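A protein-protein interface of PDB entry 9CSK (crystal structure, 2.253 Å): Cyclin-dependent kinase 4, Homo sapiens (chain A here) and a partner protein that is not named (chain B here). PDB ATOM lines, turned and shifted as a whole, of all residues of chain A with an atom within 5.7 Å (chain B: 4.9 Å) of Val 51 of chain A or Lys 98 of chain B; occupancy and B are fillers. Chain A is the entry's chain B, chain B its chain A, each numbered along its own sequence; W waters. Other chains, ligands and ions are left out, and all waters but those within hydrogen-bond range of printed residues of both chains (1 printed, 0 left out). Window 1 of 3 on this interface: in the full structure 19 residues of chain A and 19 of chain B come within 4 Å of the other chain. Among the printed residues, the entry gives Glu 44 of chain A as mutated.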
ATOM      1  N   GLU A  44      15.485   3.023  35.766  1.00  0.00           N
ATOM      2  CA  GLU A  44      15.252   2.783  34.318  1.00  0.00           C
ATOM      3  C   GLU A  44      16.586   2.598  33.588  1.00  0.00           C
ATOM      4  O   GLU A  44      16.595   2.760  32.360  1.00  0.00           O
ATOM      5  CB  GLU A  44      14.425   3.921  33.723  1.00  0.00           C
ATOM      6  CG  GLU A  44      12.994   3.938  34.227  1.00  0.00           C
ATOM      7  CD  GLU A  44      12.255   2.621  34.066  1.00  0.00           C
ATOM      8  OE1 GLU A  44      11.425   2.298  34.933  1.00  0.00           O
ATOM      9  OE2 GLU A  44      12.509   1.927  33.073  1.00  0.00           O
ATOM     10  N   GLY A  45      17.625   2.186  34.322  1.00  0.00           N
ATOM     11  CA  GLY A  45      18.979   1.925  33.793  1.00  0.00           C
ATOM     12  C   GLY A  45      19.659   3.154  33.220  1.00  0.00           C
ATOM     13  O   GLY A  45      19.716   4.175  33.921  1.00  0.00           O
ATOM     14  N   LEU A  46      20.154   3.054  31.984  1.00  0.00           N
ATOM     15  CA  LEU A  46      20.857   4.191  31.338  1.00  0.00           C
ATOM     16  C   LEU A  46      19.888   5.369  31.261  1.00  0.00           C
ATOM     17  O   LEU A  46      18.733   5.150  30.871  1.00  0.00           O
ATOM     18  CB  LEU A  46      21.274   3.773  29.926  1.00  0.00           C
ATOM     19  CG  LEU A  46      22.610   3.047  29.807  1.00  0.00           C
ATOM     20  CD1 LEU A  46      22.782   2.475  28.412  1.00  0.00           C
ATOM     21  CD2 LEU A  46      23.760   3.980  30.145  1.00  0.00           C
ATOM     22  N   PRO A  47      20.322   6.609  31.569  1.00  0.00           N
ATOM     23  CA  PRO A  47      19.437   7.765  31.502  1.00  0.00           C
ATOM     24  C   PRO A  47      18.974   7.913  30.048  1.00  0.00           C
ATOM     25  O   PRO A  47      19.787   7.797  29.159  1.00  0.00           O
ATOM     26  CB  PRO A  47      20.342   8.938  31.897  1.00  0.00           C
ATOM     27  CG  PRO A  47      21.451   8.294  32.691  1.00  0.00           C
ATOM     28  CD  PRO A  47      21.665   6.953  32.026  1.00  0.00           C
ATOM     29  N   ILE A  48      17.694   8.239  29.854  1.00  0.00           N
ATOM     30  CA  ILE A  48      17.110   8.353  28.486  1.00  0.00           C
ATOM     31  C   ILE A  48      17.848   9.442  27.700  1.00  0.00           C
ATOM     32  O   ILE A  48      18.132   9.210  26.519  1.00  0.00           O
ATOM     33  CB  ILE A  48      15.586   8.572  28.552  1.00  0.00           C
ATOM     34  CG1 ILE A  48      15.203   9.611  29.606  1.00  0.00           C
ATOM     35  CG2 ILE A  48      14.870   7.254  28.794  1.00  0.00           C
ATOM     36  CD1 ILE A  48      15.051  11.006  29.064  1.00  0.00           C
ATOM     37  N   SER A  49      18.187  10.557  28.347  1.00  0.00           N
ATOM     38  CA  SER A  49      18.926  11.655  27.675  1.00  0.00           C
ATOM     39  C   SER A  49      20.298  11.154  27.211  1.00  0.00           C
ATOM     40  O   SER A  49      20.700  11.521  26.099  1.00  0.00           O
ATOM     41  CB  SER A  49      19.049  12.842  28.588  1.00  0.00           C
ATOM     42  OG  SER A  49      17.770  13.382  28.873  1.00  0.00           O
ATOM     43  N   THR A  50      20.981  10.349  28.033  1.00  0.00           N
ATOM     44  CA  THR A  50      22.317   9.804  27.666  1.00  0.00           C
ATOM     45  C   THR A  50      22.204   8.874  26.451  1.00  0.00           C
ATOM     46  O   THR A  50      22.987   9.055  25.506  1.00  0.00           O
ATOM     47  CB  THR A  50      22.960   9.088  28.858  1.00  0.00           C
ATOM     48  OG1 THR A  50      23.144  10.054  29.891  1.00  0.00           O
ATOM     49  CG2 THR A  50      24.290   8.455  28.519  1.00  0.00           C
ATOM     50  N   VAL A  51      21.229   7.961  26.455  1.00  0.00           N
ATOM     51  CA  VAL A  51      21.009   7.080  25.326  1.00  0.00           C
ATOM     52  C   VAL A  51      20.728   7.870  24.032  1.00  0.00           C
ATOM     53  O   VAL A  51      21.439   7.637  23.062  1.00  0.00           O
ATOM     54  CB  VAL A  51      19.966   5.959  25.561  1.00  0.00           C
ATOM     55  CG1 VAL A  51      20.173   5.245  26.879  1.00  0.00           C
ATOM     56  CG2 VAL A  51      18.551   6.435  25.417  1.00  0.00           C
ATOM     57  N   ARG A  52      19.780   8.816  24.074  1.00  0.00           N
ATOM     58  CA  ARG A  52      19.384   9.660  22.908  1.00  0.00           C
ATOM     59  C   ARG A  52      20.503  10.596  22.431  1.00  0.00           C
ATOM     60  O   ARG A  52      20.751  10.628  21.218  1.00  0.00           O
ATOM     61  CB  ARG A  52      18.212  10.561  23.306  1.00  0.00           C
ATOM     62  CG  ARG A  52      16.922   9.822  23.620  1.00  0.00           C
ATOM     63  CD  ARG A  52      15.992  10.684  24.447  1.00  0.00           C
ATOM     64  NE  ARG A  52      14.704  10.047  24.654  1.00  0.00           N
ATOM     65  CZ  ARG A  52      13.738  10.536  25.415  1.00  0.00           C
ATOM     66  NH1 ARG A  52      12.600   9.879  25.539  1.00  0.00           N
ATOM     67  NH2 ARG A  52      13.909  11.680  26.048  1.00  0.00           N
ATOM     68  N   GLU A  53      21.178  11.288  23.353  1.00  0.00           N
ATOM     69  CA  GLU A  53      22.216  12.264  23.013  1.00  0.00           C
ATOM     70  C   GLU A  53      23.439  11.629  22.365  1.00  0.00           C
ATOM     71  O   GLU A  53      23.936  12.169  21.370  1.00  0.00           O
ATOM     72  CB  GLU A  53      22.627  13.098  24.219  1.00  0.00           C
ATOM     73  CG  GLU A  53      21.890  14.425  24.300  1.00  0.00           C
ATOM     74  CD  GLU A  53      22.483  15.381  25.318  1.00  0.00           C
ATOM     75  OE1 GLU A  53      22.273  16.605  25.172  1.00  0.00           O
ATOM     76  OE2 GLU A  53      23.172  14.914  26.256  1.00  0.00           O
ATOM     77  N   VAL A  54      23.964  10.557  22.961  1.00  0.00           N
ATOM     78  CA  VAL A  54      25.157   9.859  22.390  1.00  0.00           C
ATOM     79  C   VAL A  54      24.796   9.226  21.041  1.00  0.00           C
ATOM     80  O   VAL A  54      25.608   9.322  20.114  1.00  0.00           O
ATOM     81  CB  VAL A  54      25.736   8.822  23.369  1.00  0.00           C
ATOM     82  CG1 VAL A  54      26.715   7.891  22.675  1.00  0.00           C
ATOM     83  CG2 VAL A  54      26.398   9.491  24.561  1.00  0.00           C
ATOM     84  N   ALA A  55      23.619   8.607  20.946  1.00  0.00           N
ATOM     85  CA  ALA A  55      23.168   7.960  19.692  1.00  0.00           C
ATOM     86  C   ALA A  55      23.059   9.010  18.581  1.00  0.00           C
ATOM     87  O   ALA A  55      23.505   8.729  17.461  1.00  0.00           O
ATOM     88  CB  ALA A  55      21.852   7.266  19.925  1.00  0.00           C
ATOM     89  N   LEU A  56      22.503  10.179  18.898  1.00  0.00           N
ATOM     90  CA  LEU A  56      22.353  11.281  17.910  1.00  0.00           C
ATOM     91  C   LEU A  56      23.731  11.768  17.444  1.00  0.00           C
ATOM     92  O   LEU A  56      23.828  12.206  16.289  1.00  0.00           O
ATOM     93  CB  LEU A  56      21.476  12.395  18.488  1.00  0.00           C
ATOM     94  CG  LEU A  56      20.043  11.967  18.804  1.00  0.00           C
ATOM     95  CD1 LEU A  56      19.231  13.121  19.359  1.00  0.00           C
ATOM     96  CD2 LEU A  56      19.368  11.384  17.576  1.00  0.00           C
ATOM     97  N   PHE B  94      13.028  -1.818  24.867  1.00  0.00           N
ATOM     98  CA  PHE B  94      13.345  -0.847  25.890  1.00  0.00           C
ATOM     99  C   PHE B  94      14.248   0.259  25.329  1.00  0.00           C
ATOM    100  O   PHE B  94      13.948   1.429  25.523  1.00  0.00           O
ATOM    101  CB  PHE B  94      14.040  -1.594  27.041  1.00  0.00           C
ATOM    102  CG  PHE B  94      14.354  -0.804  28.286  1.00  0.00           C
ATOM    103  CD1 PHE B  94      13.353  -0.138  28.971  1.00  0.00           C
ATOM    104  CD2 PHE B  94      15.631  -0.806  28.821  1.00  0.00           C
ATOM    105  CE1 PHE B  94      13.628   0.539  30.146  1.00  0.00           C
ATOM    106  CE2 PHE B  94      15.907  -0.129  29.999  1.00  0.00           C
ATOM    107  CZ  PHE B  94      14.904   0.534  30.660  1.00  0.00           C
ATOM    108  N   VAL B  95      15.351  -0.112  24.675  1.00  0.00           N
ATOM    109  CA  VAL B  95      16.272   0.890  24.056  1.00  0.00           C
ATOM    110  C   VAL B  95      15.565   1.612  22.897  1.00  0.00           C
ATOM    111  O   VAL B  95      15.741   2.830  22.767  1.00  0.00           O
ATOM    112  CB  VAL B  95      17.593   0.244  23.605  1.00  0.00           C
ATOM    113  CG1 VAL B  95      18.526   1.269  22.983  1.00  0.00           C
ATOM    114  CG2 VAL B  95      18.283  -0.464  24.757  1.00  0.00           C
ATOM    115  N   ALA B  96      14.797   0.875  22.090  1.00  0.00           N
ATOM    116  CA  ALA B  96      14.063   1.444  20.934  1.00  0.00           C
ATOM    117  C   ALA B  96      13.020   2.454  21.424  1.00  0.00           C
ATOM    118  O   ALA B  96      12.856   3.495  20.778  1.00  0.00           O
ATOM    119  CB  ALA B  96      13.421   0.333  20.146  1.00  0.00           C
ATOM    120  N   SER B  97      12.346   2.134  22.529  1.00  0.00           N
ATOM    121  CA  SER B  97      11.321   3.027  23.124  1.00  0.00           C
ATOM    122  C   SER B  97      11.978   4.337  23.572  1.00  0.00           C
ATOM    123  O   SER B  97      11.399   5.397  23.324  1.00  0.00           O
ATOM    124  CB  SER B  97      10.646   2.338  24.274  1.00  0.00           C
ATOM    125  OG  SER B  97       9.439   2.992  24.617  1.00  0.00           O
ATOM    126  N   LYS B  98      13.160   4.257  24.184  1.00  0.00           N
ATOM    127  CA  LYS B  98      13.872   5.475  24.651  1.00  0.00           C
ATOM    128  C   LYS B  98      14.231   6.354  23.450  1.00  0.00           C
ATOM    129  O   LYS B  98      14.062   7.575  23.543  1.00  0.00           O
ATOM    130  CB  LYS B  98      15.160   5.081  25.375  1.00  0.00           C
ATOM    131  CG  LYS B  98      14.976   4.225  26.617  1.00  0.00           C
ATOM    132  CD  LYS B  98      16.215   4.137  27.465  1.00  0.00           C
ATOM    133  CE  LYS B  98      15.953   3.512  28.817  1.00  0.00           C
ATOM    134  NZ  LYS B  98      17.200   3.359  29.600  1.00  0.00           N
ATOM    135  N   MET B  99      14.721   5.730  22.378  1.00  0.00           N
ATOM    136  CA  MET B  99      15.147   6.425  21.134  1.00  0.00           C
ATOM    137  C   MET B  99      13.976   7.068  20.380  1.00  0.00           C
ATOM    138  O   MET B  99      14.163   8.189  19.890  1.00  0.00           O
ATOM    139  CB  MET B  99      15.857   5.446  20.197  1.00  0.00           C
ATOM    140  CG  MET B  99      17.273   5.146  20.616  1.00  0.00           C
ATOM    141  SD  MET B  99      18.259   6.641  20.793  1.00  0.00           S
ATOM    142  CE  MET B  99      18.105   7.333  19.149  1.00  0.00           C
ATOM    143  N   LYS B 100      12.828   6.388  20.290  1.00  0.00           N
ATOM    144  CA  LYS B 100      11.699   6.894  19.463  1.00  0.00           C
ATOM    145  C   LYS B 100      10.473   7.376  20.251  1.00  0.00           C
ATOM    146  O   LYS B 100       9.518   7.778  19.578  1.00  0.00           O
ATOM    147  CB  LYS B 100      11.237   5.793  18.505  1.00  0.00           C
ATOM    148  CG  LYS B 100      12.233   5.395  17.426  1.00  0.00           C
ATOM    149  CD  LYS B 100      12.512   6.496  16.433  1.00  0.00           C
ATOM    150  CE  LYS B 100      13.609   6.152  15.452  1.00  0.00           C
ATOM    151  NZ  LYS B 100      13.907   7.284  14.548  1.00  0.00           N
ATOM    152  N   GLU B 101      10.468   7.394  21.585  1.00  0.00           N
ATOM    153  CA  GLU B 101       9.192   7.805  22.241  1.00  0.00           C
ATOM    154  C   GLU B 101       9.364   8.923  23.273  1.00  0.00           C
ATOM    155  O   GLU B 101      10.431   8.996  23.898  1.00  0.00           O
ATOM    156  CB  GLU B 101       8.459   6.610  22.853  1.00  0.00           C
ATOM    157  CG  GLU B 101       7.886   5.666  21.818  1.00  0.00           C
ATOM    158  CD  GLU B 101       7.023   4.552  22.373  1.00  0.00           C
ATOM    159  OE1 GLU B 101       7.566   3.663  23.042  1.00  0.00           O
ATOM    160  OE2 GLU B 101       5.812   4.579  22.131  1.00  0.00           O
ATOM    161  N   PRO B 104       9.101   6.692  27.203  1.00  0.00           N
ATOM    162  CA  PRO B 104       9.616   5.356  26.928  1.00  0.00           C
ATOM    163  C   PRO B 104       8.973   4.290  27.827  1.00  0.00           C
ATOM    164  O   PRO B 104       8.582   4.606  28.929  1.00  0.00           O
ATOM    165  CB  PRO B 104      11.115   5.474  27.234  1.00  0.00           C
ATOM    166  CG  PRO B 104      11.385   6.953  27.212  1.00  0.00           C
ATOM    167  CD  PRO B 104      10.119   7.570  27.762  1.00  0.00           C
ATOM    168  N   GLU B 127      20.721  -4.085  28.911  1.00  0.00           N
ATOM    169  CA  GLU B 127      20.787  -2.790  28.228  1.00  0.00           C
ATOM    170  C   GLU B 127      22.224  -2.365  27.991  1.00  0.00           C
ATOM    171  O   GLU B 127      22.541  -1.878  26.908  1.00  0.00           O
ATOM    172  CB  GLU B 127      20.035  -1.709  29.010  1.00  0.00           C
ATOM    173  CG  GLU B 127      20.090  -0.357  28.334  1.00  0.00           C
ATOM    174  CD  GLU B 127      19.446   0.783  29.095  1.00  0.00           C
ATOM    175  OE1 GLU B 127      19.692   0.909  30.319  1.00  0.00           O
ATOM    176  OE2 GLU B 127      18.710   1.569  28.452  1.00  0.00           O
ATOM    177  N   TRP B 136      26.739   1.969  20.515  1.00  0.00           N
ATOM    178  CA  TRP B 136      25.778   3.056  20.672  1.00  0.00           C
ATOM    179  C   TRP B 136      25.277   3.595  19.337  1.00  0.00           C
ATOM    180  O   TRP B 136      24.969   4.780  19.242  1.00  0.00           O
ATOM    181  CB  TRP B 136      26.288   4.164  21.582  1.00  0.00           C
ATOM    182  CG  TRP B 136      26.531   3.725  22.998  1.00  0.00           C
ATOM    183  CD1 TRP B 136      27.412   2.771  23.427  1.00  0.00           C
ATOM    184  CD2 TRP B 136      25.966   4.309  24.178  1.00  0.00           C
ATOM    185  NE1 TRP B 136      27.399   2.701  24.798  1.00  0.00           N
ATOM    186  CE2 TRP B 136      26.539   3.653  25.286  1.00  0.00           C
ATOM    187  CE3 TRP B 136      25.060   5.348  24.405  1.00  0.00           C
ATOM    188  CZ2 TRP B 136      26.247   4.017  26.606  1.00  0.00           C
ATOM    189  CZ3 TRP B 136      24.786   5.719  25.708  1.00  0.00           C
ATOM    190  CH2 TRP B 136      25.366   5.051  26.791  1.00  0.00           C
ATOM    191  N   LEU B 138      22.414   3.652  17.877  1.00  0.00           N
ATOM    192  CA  LEU B 138      21.022   3.398  18.206  1.00  0.00           C
ATOM    193  C   LEU B 138      20.038   4.147  17.319  1.00  0.00           C
ATOM    194  O   LEU B 138      18.901   3.701  17.151  1.00  0.00           O
ATOM    195  CB  LEU B 138      20.776   3.691  19.688  1.00  0.00           C
ATOM    196  CG  LEU B 138      21.776   3.091  20.693  1.00  0.00           C
ATOM    197  CD1 LEU B 138      21.484   3.588  22.125  1.00  0.00           C
ATOM    198  CD2 LEU B 138      21.800   1.587  20.619  1.00  0.00           C
HETATM  199  O   HOH W   1      23.298   6.375  16.534  1.00  0.00           O
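Glu 44 of chain A touches Phe 94 of chain B (O to CZ, 3.3 Å). Gly 45 of chain A touches Glu 127 of chain B (C to OE1, 3.7 Å). CH2 of Trp 136 of chain B touches CD2 of Leu 46 of chain A, at 3.9 Å. CD of Lys 98 of chain B touches CG2 of Ile 48 of chain A, 3.6 Å away. Trp 136 of chain B touches Thr 50 of chain A. Lys 98 of chain B touches Val 51 of chain A. Met 99 of chain B touches Arg 52 of chain A (SD to CA, 3.9 Å). CG of Pro 104 of chain B touches NH1 of Arg 52 of chain A, 3.6 Å away. CG1 of Val 54 of chain A touches CE3 of Trp 136 of chain B, 3.5 Å away. CB of Ala 55 of chain A touches SD of Met 99 of chain B (3.7 Å).
Of the 13 printed residues of chain A, 9 touch a printed residue of chain B. Hydrophobic or aromatic side chains of chain A within 4 Å of the printed part of chain B: Leu 46, Ile 48, Val 51, Val 54 and Ala 55. Among the printed residues, no Asp or Glu carboxylate lies within 4 Å of a Lys or Arg side-chain nitrogen of the other chain.
The side-chain carboxylate of Glu 101 of chain B sits at hydrogen-bond distance from the side-chain hydroxyl of Ser 97 of chain B. The side-chain carboxylate of Glu 127 of chain B lies within salt-bridge range of the side-chain amino group of Lys 98 of chain B, at 2.6 Å.
Water W1 bridges O of Ala 55 of chain A (2.5 Å) and N of Leu 138 of chain B (3.2 Å).
The side-chain amino group (NZ) of Lys 98 of chain B is in hydrogen-bond range of the backbone carbonyl oxygen (O) of Glu 44 of chain A, 2.9 Å away. NZ of Lys 98 of chain B sits at hydrogen-bond distance from O of Leu 46 of chain A (2.7 Å). O of Lys 98 of chain B lies within hydrogen-bond range of NE of Arg 52 of chain A (2.8 Å). O of Glu 101 of chain B is in hydrogen-bond range of NH1 of Arg 52 of chain A (2.9 Å). The backbone NH of Leu 46 of chain A sits at hydrogen-bond distance from the side-chain carboxylate of Glu 127 of chain B, 2.8 Å away.
Of the printed residues of chain B, Glu 44 of chain A touches Phe 94 (3.3 Å) and Lys 98 (2.9 Å). Of the printed residues of chain B, Thr 50 of chain A touches Trp 136 (3.8 Å). Val 51 of chain A touches just one residue of chain B: Lys 98. Glu 53 of chain A touches none of the printed residues of chain B. Of the printed residues of chain B, Val 54 of chain A touches Trp 136 (3.5 Å). Of the printed residues of chain A, Met 99 of chain B touches Arg 52 (3.9 Å) and Ala 55 (3.7 Å). Printed residues of chain A within 4 Å of Leu 138 of chain B: Ala 55 (3.7 Å). The nearest residue of chain A that does not touch Lys 98 of chain B is Gly 45 of chain A (4.4 Å). The nearest printed residue of chain A that does not touch Phe 94 of chain B is Gly 45 of chain A (4.9 Å).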
